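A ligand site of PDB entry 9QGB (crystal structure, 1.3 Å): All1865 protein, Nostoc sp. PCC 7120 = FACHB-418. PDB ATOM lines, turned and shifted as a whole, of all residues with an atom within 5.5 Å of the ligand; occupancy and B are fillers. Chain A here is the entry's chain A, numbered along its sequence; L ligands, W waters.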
ATOM      1  N   ALA A  35      -2.770 -28.262  13.881  1.00  0.00           N
ATOM      2  CA  ALA A  35      -2.298 -28.883  12.636  1.00  0.00           C
ATOM      3  C   ALA A  35      -1.612 -30.207  12.961  1.00  0.00           C
ATOM      4  O   ALA A  35      -1.051 -30.390  14.056  1.00  0.00           O
ATOM      5  CB  ALA A  35      -1.287 -27.936  11.943  1.00  0.00           C
ATOM      6  N   PRO A  36      -1.546 -31.119  11.979  1.00  0.00           N
ATOM      7  CA  PRO A  36      -0.815 -32.357  12.168  1.00  0.00           C
ATOM      8  C   PRO A  36       0.688 -32.102  12.290  1.00  0.00           C
ATOM      9  O   PRO A  36       1.283 -31.357  11.465  1.00  0.00           O
ATOM     10  CB  PRO A  36      -1.155 -33.197  10.905  1.00  0.00           C
ATOM     11  CG  PRO A  36      -1.459 -32.108   9.861  1.00  0.00           C
ATOM     12  CD  PRO A  36      -2.152 -31.011  10.646  1.00  0.00           C
ATOM     13  N   LEU A  37       1.312 -32.700  13.310  1.00  0.00           N
ATOM     14  CA  LEU A  37       2.719 -32.452  13.614  1.00  0.00           C
ATOM     15  C   LEU A  37       3.419 -33.758  13.949  1.00  0.00           C
ATOM     16  O   LEU A  37       3.239 -34.304  15.059  1.00  0.00           O
ATOM     17  CB  LEU A  37       2.872 -31.468  14.780  1.00  0.00           C
ATOM     18  CG  LEU A  37       2.283 -30.064  14.538  1.00  0.00           C
ATOM     19  CD1 LEU A  37       1.884 -29.450  15.857  1.00  0.00           C
ATOM     20  CD2 LEU A  37       3.268 -29.209  13.761  1.00  0.00           C
ATOM     21  N   THR A  38       4.239 -34.237  13.009  1.00  0.00           N
ATOM     22  CA  THR A  38       5.118 -35.386  13.265  1.00  0.00           C
ATOM     23  C   THR A  38       6.050 -35.092  14.446  1.00  0.00           C
ATOM     24  O   THR A  38       6.804 -34.095  14.414  1.00  0.00           O
ATOM     25  CB  THR A  38       5.915 -35.669  11.986  1.00  0.00           C
ATOM     26  OG1 THR A  38       5.024 -36.168  10.972  1.00  0.00           O
ATOM     27  CG2 THR A  38       7.045 -36.666  12.150  1.00  0.00           C
ATOM     28  N   ARG A  39       6.029 -35.936  15.478  1.00  0.00           N
ATOM     29  CA  ARG A  39       6.910 -35.747  16.622  1.00  0.00           C
ATOM     30  C   ARG A  39       7.861 -36.938  16.828  1.00  0.00           C
ATOM     31  O   ARG A  39       8.726 -36.869  17.712  1.00  0.00           O
ATOM     32  CB  ARG A  39       6.119 -35.474  17.920  1.00  0.00           C
ATOM     33  CG  ARG A  39       5.098 -34.343  17.780  1.00  0.00           C
ATOM     34  CD  ARG A  39       5.679 -32.993  17.371  1.00  0.00           C
ATOM     35  NE  ARG A  39       6.798 -32.551  18.218  1.00  0.00           N
ATOM     36  CZ  ARG A  39       6.591 -31.943  19.403  1.00  0.00           C
ATOM     37  NH1 ARG A  39       7.637 -31.654  20.194  1.00  0.00           N
ATOM     38  NH2 ARG A  39       5.358 -31.620  19.809  1.00  0.00           N
ATOM     39  N   GLU A  68      -0.754 -36.210  14.259  1.00  0.00           N
ATOM     40  CA  GLU A  68       0.426 -36.372  13.388  1.00  0.00           C
ATOM     41  C   GLU A  68       0.170 -37.385  12.296  1.00  0.00           C
ATOM     42  O   GLU A  68      -0.570 -38.364  12.443  1.00  0.00           O
ATOM     43  CB  GLU A  68       1.595 -36.813  14.268  1.00  0.00           C
ATOM     44  CG  GLU A  68       1.399 -38.224  14.834  1.00  0.00           C
ATOM     45  CD  GLU A  68       2.162 -38.391  16.131  1.00  0.00           C
ATOM     46  OE1 GLU A  68       3.376 -38.682  16.064  1.00  0.00           O
ATOM     47  OE2 GLU A  68       1.571 -38.245  17.222  1.00  0.00           O
ATOM     48  N   ALA A  69       0.886 -37.168  11.185  1.00  0.00           N
ATOM     49  CA  ALA A  69       0.857 -38.147  10.096  1.00  0.00           C
ATOM     50  C   ALA A  69       1.166 -39.560  10.626  1.00  0.00           C
ATOM     51  O   ALA A  69       2.145 -39.778  11.346  1.00  0.00           O
ATOM     52  CB  ALA A  69       1.886 -37.752   9.056  1.00  0.00           C
ATOM     53  N   GLN A 111      -4.465 -38.113  10.958  1.00  0.00           N
ATOM     54  CA  GLN A 111      -3.961 -37.910   9.599  1.00  0.00           C
ATOM     55  C   GLN A 111      -3.367 -39.224   9.067  1.00  0.00           C
ATOM     56  O   GLN A 111      -2.426 -39.799   9.648  1.00  0.00           O
ATOM     57  CB  GLN A 111      -2.954 -36.762   9.563  1.00  0.00           C
ATOM     58  CG  GLN A 111      -2.667 -36.363   8.116  1.00  0.00           C
ATOM     59  CD  GLN A 111      -1.523 -35.414   7.942  1.00  0.00           C
ATOM     60  OE1 GLN A 111      -0.426 -35.683   8.442  1.00  0.00           O
ATOM     61  NE2 GLN A 111      -1.781 -34.326   7.215  1.00  0.00           N
ATOM     62  N   GLU A 185      -8.066 -37.452   8.404  1.00  0.00           N
ATOM     63  CA  GLU A 185      -7.610 -36.529   7.375  1.00  0.00           C
ATOM     64  C   GLU A 185      -6.705 -37.296   6.422  1.00  0.00           C
ATOM     65  O   GLU A 185      -5.749 -37.936   6.831  1.00  0.00           O
ATOM     66  CB  GLU A 185      -6.830 -35.342   7.980  1.00  0.00           C
ATOM     67  CG  GLU A 185      -6.370 -34.359   6.903  1.00  0.00           C
ATOM     68  CD  GLU A 185      -5.655 -33.172   7.528  1.00  0.00           C
ATOM     69  OE1 GLU A 185      -4.418 -33.157   7.588  1.00  0.00           O
ATOM     70  OE2 GLU A 185      -6.351 -32.200   7.914  1.00  0.00           O
ATOM     71  N   HIS A 187      -3.701 -37.400   4.066  1.00  0.00           N
ATOM     72  CA  HIS A 187      -2.527 -36.567   3.815  1.00  0.00           C
ATOM     73  C   HIS A 187      -2.214 -36.599   2.322  1.00  0.00           C
ATOM     74  O   HIS A 187      -1.538 -37.494   1.814  1.00  0.00           O
ATOM     75  CB  HIS A 187      -1.336 -37.069   4.640  1.00  0.00           C
ATOM     76  CG  HIS A 187      -0.209 -36.076   4.658  1.00  0.00           C
ATOM     77  ND1 HIS A 187       0.867 -36.057   5.530  1.00  0.00           N
ATOM     78  CD2 HIS A 187      -0.109 -34.967   3.872  1.00  0.00           C
ATOM     79  CE1 HIS A 187       1.611 -34.984   5.232  1.00  0.00           C
ATOM     80  NE2 HIS A 187       0.993 -34.338   4.247  1.00  0.00           N
ATOM     81  N   ALA A 189      -0.620 -33.974   0.866  1.00  0.00           N
ATOM     82  CA  ALA A 189       0.232 -32.804   0.830  1.00  0.00           C
ATOM     83  C   ALA A 189       1.698 -33.181   1.026  1.00  0.00           C
ATOM     84  O   ALA A 189       2.065 -34.379   1.161  1.00  0.00           O
ATOM     85  CB  ALA A 189      -0.221 -31.840   1.924  1.00  0.00           C
ATOM     86  N   ASN A 190       2.542 -32.144   1.047  1.00  0.00           N
ATOM     87  CA  ASN A 190       3.966 -32.151   1.423  1.00  0.00           C
ATOM     88  C   ASN A 190       4.801 -33.184   0.667  1.00  0.00           C
ATOM     89  O   ASN A 190       5.858 -33.579   1.168  1.00  0.00           O
ATOM     90  CB  ASN A 190       4.121 -32.279   2.937  1.00  0.00           C
ATOM     91  CG  ASN A 190       3.463 -31.102   3.639  1.00  0.00           C
ATOM     92  OD1 ASN A 190       3.247 -30.049   3.018  1.00  0.00           O
ATOM     93  ND2 ASN A 190       3.178 -31.223   4.931  1.00  0.00           N
ATOM     94  N   ARG A 239      -6.027 -32.977   3.075  1.00  0.00           N
ATOM     95  CA  ARG A 239      -5.036 -31.893   3.157  1.00  0.00           C
ATOM     96  C   ARG A 239      -4.248 -31.805   1.844  1.00  0.00           C
ATOM     97  O   ARG A 239      -3.760 -32.832   1.348  1.00  0.00           O
ATOM     98  CB  ARG A 239      -4.061 -32.112   4.320  1.00  0.00           C
ATOM     99  CG  ARG A 239      -3.317 -30.804   4.617  1.00  0.00           C
ATOM    100  CD  ARG A 239      -2.437 -30.906   5.877  1.00  0.00           C
ATOM    101  NE  ARG A 239      -2.246 -29.562   6.443  1.00  0.00           N
ATOM    102  CZ  ARG A 239      -1.246 -29.160   7.236  1.00  0.00           C
ATOM    103  NH1 ARG A 239      -0.132 -29.860   7.334  1.00  0.00           N
ATOM    104  NH2 ARG A 239      -1.379 -28.023   7.907  1.00  0.00           N
ATOM    105  N   PHE A 276      -2.418 -26.185   3.466  1.00  0.00           N
ATOM    106  CA  PHE A 276      -1.193 -25.626   4.013  1.00  0.00           C
ATOM    107  C   PHE A 276      -0.641 -24.684   2.929  1.00  0.00           C
ATOM    108  O   PHE A 276      -0.278 -25.117   1.819  1.00  0.00           O
ATOM    109  CB  PHE A 276      -0.206 -26.780   4.235  1.00  0.00           C
ATOM    110  CG  PHE A 276       1.233 -26.367   4.550  1.00  0.00           C
ATOM    111  CD1 PHE A 276       1.597 -25.123   5.026  1.00  0.00           C
ATOM    112  CD2 PHE A 276       2.242 -27.333   4.384  1.00  0.00           C
ATOM    113  CE1 PHE A 276       2.952 -24.840   5.265  1.00  0.00           C
ATOM    114  CE2 PHE A 276       3.563 -27.081   4.699  1.00  0.00           C
ATOM    115  CZ  PHE A 276       3.910 -25.815   5.114  1.00  0.00           C
ATOM    116  N   ILE A 279       5.016 -21.338   3.135  1.00  0.00           N
ATOM    117  CA  ILE A 279       5.448 -20.098   3.767  1.00  0.00           C
ATOM    118  C   ILE A 279       6.136 -19.159   2.772  1.00  0.00           C
ATOM    119  O   ILE A 279       6.124 -17.953   2.981  1.00  0.00           O
ATOM    120  CB  ILE A 279       6.317 -20.388   4.996  1.00  0.00           C
ATOM    121  CG1 ILE A 279       5.501 -21.130   6.089  1.00  0.00           C
ATOM    122  CG2 ILE A 279       6.924 -19.105   5.569  1.00  0.00           C
ATOM    123  CD1 ILE A 279       4.070 -20.656   6.320  1.00  0.00           C
ATOM    124  N   ASN A 306      -3.833 -22.703   6.773  1.00  0.00           N
ATOM    125  CA  ASN A 306      -2.701 -22.928   7.654  1.00  0.00           C
ATOM    126  C   ASN A 306      -1.462 -22.311   7.025  1.00  0.00           C
ATOM    127  O   ASN A 306      -1.340 -22.301   5.790  1.00  0.00           O
ATOM    128  CB  ASN A 306      -2.525 -24.435   7.874  1.00  0.00           C
ATOM    129  CG  ASN A 306      -1.139 -24.751   8.378  1.00  0.00           C
ATOM    130  OD1 ASN A 306      -0.242 -25.033   7.558  1.00  0.00           O
ATOM    131  ND2 ASN A 306      -0.923 -24.666   9.690  1.00  0.00           N
ATOM    132  N   GLY A 307      -0.522 -21.881   7.893  1.00  0.00           N
ATOM    133  CA  GLY A 307       0.798 -21.477   7.445  1.00  0.00           C
ATOM    134  C   GLY A 307       1.114 -20.082   7.959  1.00  0.00           C
ATOM    135  O   GLY A 307       0.690 -19.097   7.357  1.00  0.00           O
ATOM    136  N   GLY A 308       1.808 -20.001   9.111  1.00  0.00           N
ATOM    137  CA  GLY A 308       2.198 -18.694   9.639  1.00  0.00           C
ATOM    138  C   GLY A 308       1.058 -17.882  10.277  1.00  0.00           C
ATOM    139  O   GLY A 308       1.166 -16.658  10.392  1.00  0.00           O
ATOM    140  N   TYR A 309      -0.079 -18.485  10.631  1.00  0.00           N
ATOM    141  CA  TYR A 309      -1.179 -17.714  11.176  1.00  0.00           C
ATOM    142  C   TYR A 309      -0.886 -17.223  12.601  1.00  0.00           C
ATOM    143  O   TYR A 309      -0.060 -17.745  13.356  1.00  0.00           O
ATOM    144  CB  TYR A 309      -2.522 -18.469  11.094  1.00  0.00           C
ATOM    145  CG  TYR A 309      -3.045 -18.353   9.683  1.00  0.00           C
ATOM    146  CD1 TYR A 309      -2.601 -19.219   8.682  1.00  0.00           C
ATOM    147  CD2 TYR A 309      -3.951 -17.336   9.337  1.00  0.00           C
ATOM    148  CE1 TYR A 309      -3.031 -19.079   7.372  1.00  0.00           C
ATOM    149  CE2 TYR A 309      -4.366 -17.196   8.027  1.00  0.00           C
ATOM    150  CZ  TYR A 309      -3.888 -18.049   7.044  1.00  0.00           C
ATOM    151  OH  TYR A 309      -4.303 -17.891   5.744  1.00  0.00           O
ATOM    152  N   ALA A 327      -5.677 -23.561  11.200  1.00  0.00           N
ATOM    153  CA  ALA A 327      -4.818 -24.509  11.903  1.00  0.00           C
ATOM    154  C   ALA A 327      -3.462 -23.887  12.188  1.00  0.00           C
ATOM    155  O   ALA A 327      -2.875 -23.216  11.330  1.00  0.00           O
ATOM    156  CB  ALA A 327      -4.700 -25.784  11.067  1.00  0.00           C
ATOM    157  N   PHE A 328      -2.973 -24.150  13.388  1.00  0.00           N
ATOM    158  CA  PHE A 328      -1.670 -23.705  13.872  1.00  0.00           C
ATOM    159  C   PHE A 328      -0.830 -24.938  14.136  1.00  0.00           C
ATOM    160  O   PHE A 328      -1.274 -25.864  14.834  1.00  0.00           O
ATOM    161  CB  PHE A 328      -1.836 -22.920  15.172  1.00  0.00           C
ATOM    162  CG  PHE A 328      -2.683 -21.665  15.016  1.00  0.00           C
ATOM    163  CD1 PHE A 328      -4.080 -21.718  15.004  1.00  0.00           C
ATOM    164  CD2 PHE A 328      -2.080 -20.421  14.905  1.00  0.00           C
ATOM    165  CE1 PHE A 328      -4.824 -20.532  14.890  1.00  0.00           C
ATOM    166  CE2 PHE A 328      -2.805 -19.254  14.807  1.00  0.00           C
ATOM    167  CZ  PHE A 328      -4.175 -19.313  14.826  1.00  0.00           C
ATOM    168  N   GLY A 329       0.414 -24.910  13.607  1.00  0.00           N
ATOM    169  CA  GLY A 329       1.362 -25.981  13.823  1.00  0.00           C
ATOM    170  C   GLY A 329       2.336 -25.604  14.914  1.00  0.00           C
ATOM    171  O   GLY A 329       2.193 -26.008  16.079  1.00  0.00           O
ATOM    172  N   THR A 330       3.346 -24.823  14.526  1.00  0.00           N
ATOM    173  CA  THR A 330       4.445 -24.483  15.414  1.00  0.00           C
ATOM    174  C   THR A 330       3.927 -23.982  16.775  1.00  0.00           C
ATOM    175  O   THR A 330       4.426 -24.389  17.841  1.00  0.00           O
ATOM    176  CB  THR A 330       5.338 -23.419  14.735  1.00  0.00           C
ATOM    177  OG1 THR A 330       5.779 -23.936  13.488  1.00  0.00           O
ATOM    178  CG2 THR A 330       6.545 -23.099  15.596  1.00  0.00           C
ATOM    179  N   LEU A 331       2.956 -23.047  16.767  1.00  0.00           N
ATOM    180  CA  LEU A 331       2.501 -22.483  18.054  1.00  0.00           C
ATOM    181  C   LEU A 331       1.850 -23.521  18.958  1.00  0.00           C
ATOM    182  O   LEU A 331       1.903 -23.375  20.178  1.00  0.00           O
ATOM    183  CB  LEU A 331       1.539 -21.307  17.895  1.00  0.00           C
ATOM    184  CG  LEU A 331       2.200 -20.031  17.411  1.00  0.00           C
ATOM    185  CD1 LEU A 331       1.142 -18.996  17.136  1.00  0.00           C
ATOM    186  CD2 LEU A 331       3.150 -19.529  18.504  1.00  0.00           C
ATOM    187  N   ILE A 333       2.934 -26.651  19.196  1.00  0.00           N
ATOM    188  CA  ILE A 333       4.024 -27.383  19.815  1.00  0.00           C
ATOM    189  C   ILE A 333       4.353 -26.762  21.168  1.00  0.00           C
ATOM    190  O   ILE A 333       4.406 -27.460  22.204  1.00  0.00           O
ATOM    191  CB  ILE A 333       5.300 -27.397  18.943  1.00  0.00           C
ATOM    192  CG1 ILE A 333       5.003 -28.189  17.677  1.00  0.00           C
ATOM    193  CG2 ILE A 333       6.521 -27.947  19.711  1.00  0.00           C
ATOM    194  CD1 ILE A 333       6.154 -28.168  16.678  1.00  0.00           C
ATOM    195  N   PHE A 356      11.677 -30.939  18.368  1.00  0.00           N
ATOM    196  CA  PHE A 356      10.495 -31.253  17.578  1.00  0.00           C
ATOM    197  C   PHE A 356      10.412 -32.732  17.285  1.00  0.00           C
ATOM    198  O   PHE A 356       9.348 -33.355  17.464  1.00  0.00           O
ATOM    199  CB  PHE A 356      10.454 -30.513  16.234  1.00  0.00           C
ATOM    200  CG  PHE A 356      10.153 -29.027  16.325  1.00  0.00           C
ATOM    201  CD1 PHE A 356       9.850 -28.413  17.562  1.00  0.00           C
ATOM    202  CD2 PHE A 356      10.173 -28.227  15.164  1.00  0.00           C
ATOM    203  CE1 PHE A 356       9.568 -27.041  17.633  1.00  0.00           C
ATOM    204  CE2 PHE A 356       9.864 -26.874  15.206  1.00  0.00           C
ATOM    205  CZ  PHE A 356       9.583 -26.281  16.441  1.00  0.00           C
ATOM    206  N   TYR A 357      11.525 -33.343  16.843  1.00  0.00           N
ATOM    207  CA  TYR A 357      11.450 -34.705  16.332  1.00  0.00           C
ATOM    208  C   TYR A 357      12.227 -35.659  17.235  1.00  0.00           C
ATOM    209  O   TYR A 357      13.449 -35.503  17.371  1.00  0.00           O
ATOM    210  CB  TYR A 357      12.075 -34.781  14.943  1.00  0.00           C
ATOM    211  CG  TYR A 357      11.360 -33.953  13.896  1.00  0.00           C
ATOM    212  CD1 TYR A 357      10.093 -34.369  13.422  1.00  0.00           C
ATOM    213  CD2 TYR A 357      11.922 -32.795  13.357  1.00  0.00           C
ATOM    214  CE1 TYR A 357       9.428 -33.678  12.418  1.00  0.00           C
ATOM    215  CE2 TYR A 357      11.206 -32.050  12.401  1.00  0.00           C
ATOM    216  CZ  TYR A 357       9.988 -32.525  11.908  1.00  0.00           C
ATOM    217  OH  TYR A 357       9.338 -31.904  10.866  1.00  0.00           O
HETATM  218  N1  LIG L   1       2.208 -31.457   8.085  1.00  0.00           N
HETATM  219  C1  LIG L   1       1.428 -32.558   7.890  1.00  0.00           C
HETATM  220  O1  LIG L   1       0.530 -32.563   7.014  1.00  0.00           O
HETATM  221  N2  LIG L   1       1.591 -33.702   8.636  1.00  0.00           N
HETATM  222  C2  LIG L   1       2.566 -33.778   9.618  1.00  0.00           C
HETATM  223  O2  LIG L   1       2.672 -34.832  10.304  1.00  0.00           O
HETATM  224  C3  LIG L   1       3.469 -32.665   9.773  1.00  0.00           C
HETATM  225  N3  LIG L   1       4.486 -32.745  10.636  1.00  0.00           N
HETATM  226  C4  LIG L   1       5.116 -31.568  11.007  1.00  0.00           C
HETATM  227  C5  LIG L   1       6.089 -31.605  12.043  1.00  0.00           C
HETATM  228  C6  LIG L   1       6.701 -30.437  12.473  1.00  0.00           C
HETATM  229  C7  LIG L   1       7.674 -30.481  13.626  1.00  0.00           C
HETATM  230  C8  LIG L   1       6.400 -29.216  11.815  1.00  0.00           C
HETATM  231  C9  LIG L   1       7.020 -27.924  12.288  1.00  0.00           C
HETATM  232  C10 LIG L   1       5.520 -29.207  10.746  1.00  0.00           C
HETATM  233  C11 LIG L   1       4.837 -30.353  10.339  1.00  0.00           C
HETATM  234  N4  LIG L   1       3.869 -30.351   9.325  1.00  0.00           N
HETATM  235  C12 LIG L   1       3.136 -31.490   9.032  1.00  0.00           C
HETATM  236  C13 LIG L   1       3.424 -29.102   8.720  1.00  0.00           C
HETATM  237  C14 LIG L   1       2.500 -28.367   9.751  1.00  0.00           C
HETATM  238  O3  LIG L   1       1.243 -29.088   9.903  1.00  0.00           O
HETATM  239  C15 LIG L   1       2.100 -26.956   9.310  1.00  0.00           C
HETATM  240  O4  LIG L   1       1.410 -27.073   8.074  1.00  0.00           O
HETATM  241  C16 LIG L   1       3.293 -26.022   9.123  1.00  0.00           C
HETATM  242  O5  LIG L   1       4.174 -26.110  10.254  1.00  0.00           O
HETATM  243  C17 LIG L   1       2.861 -24.601   8.871  1.00  0.00           C
HETATM  244  O6  LIG L   1       1.980 -24.093   9.903  1.00  0.00           O
HETATM  245  P1  LIG L   1       2.574 -23.190  11.114  1.00  0.00           P
HETATM  246  O7  LIG L   1       1.322 -22.920  11.933  1.00  0.00           O
HETATM  247  O8  LIG L   1       3.194 -21.961  10.465  1.00  0.00           O
HETATM  248  O9  LIG L   1       3.582 -24.045  11.854  1.00  0.00           O
HETATM  249  O   HOH W   1       6.736 -25.808   9.013  1.00  0.00           O
HETATM  250  O   HOH W   2       4.140 -20.070  12.206  1.00  0.00           O
HETATM  251  O   HOH W   3       1.681 -21.833  14.460  1.00  0.00           O
HETATM  252  O   HOH W   4       5.671 -21.511   9.539  1.00  0.00           O
HETATM  253  O   HOH W   5      -0.685 -21.450  10.767  1.00  0.00           O
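O9 of the ligand lies within hydrogen-bond range of OG1 of Thr 330, 2.7 Å away.
N of Thr 330 sits at hydrogen-bond distance from O9 of the ligand (2.8 Å).
The backbone NH of Ala 69 is in hydrogen-bond range of an oxygen (O2) of the ligand, 3.1 Å away.
The side-chain amide oxygen of Asn 306 sits at hydrogen-bond distance from an oxygen (O4) of the ligand (2.7 Å).
An oxygen (O2) of the ligand lies within hydrogen-bond range of the side-chain hydroxyl (OG1) of Thr 38 (2.8 Å).
NE2 of His 187 lies close to O1 of the ligand (3.3 Å).
ND2 of Asn 190 lies within hydrogen-bond range of N1 of the ligand (3.3 Å).
The side-chain amide oxygen of Gln 111 sits at hydrogen-bond distance from a nitrogen (N2) of the ligand (2.8 Å).
The backbone NH (N) of Gly 308 lies within hydrogen-bond range of an oxygen (O8) of the ligand, 2.8 Å away.
O of Pro 36 lies within hydrogen-bond range of O3 of the ligand.
O7 of the ligand sits at hydrogen-bond distance from N of Gly 329.
NH1 of Arg 239 is in hydrogen-bond range of O1 of the ligand.
A nitrogen (N3) of the ligand is in hydrogen-bond range of the backbone NH (N) of Thr 38.
A ring nitrogen (NE2) of His 187 is in hydrogen-bond range of the backbone carbonyl oxygen of Ala 189 (3.3 Å).
OE1 of Gln 111 sits at hydrogen-bond distance from ND1 of His 187.
The guanidinium group (NE) of Arg 39 is in hydrogen-bond range of the backbone carbonyl oxygen (O) of Phe 356.
The backbone NH (N) of Ala 189 sits at hydrogen-bond distance from the backbone carbonyl oxygen (O) of Arg 239, 3.4 Å away.
OE1 of Gln 111 lies close to N of Ala 69, 3.4 Å away.
ND2 of Asn 306 sits at hydrogen-bond distance from O of Ala 327 (2.9 Å).
NE2 of Gln 111 lies within hydrogen-bond range of OE1 of Glu 185.
N of Ala 35 is in hydrogen-bond range of O of Phe 328 (3.0 Å).
Ala 35 touches the ligand.
Leu 37 touches the ligand (CA to N3, 3.5 Å).
CG of Phe 276 touches O4 of the ligand (3.6 Å).
Gly 307 touches the ligand.
Phe 328 touches the ligand.
Phe 356 touches the ligand (CD2 to C7, 3.7 Å).
Tyr 357 touches the ligand (OH to C6, 3.4 Å).
Hydrophobic or aromatic side chains within 4 Å of the ligand: Ala 35, Pro 36, Leu 37, Ala 69, His 187, Phe 276, Phe 356 and Tyr 357.
18 residues have an atom within 4 Å of the ligand: Ala 35, Pro 36, Leu 37, Thr 38, Ala 69, Gln 111, His 187, Asn 190, Arg 239, Phe 276, Asn 306, Gly 307, Gly 308, Phe 328, Gly 329, Thr 330, Phe 356 and Tyr 357.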
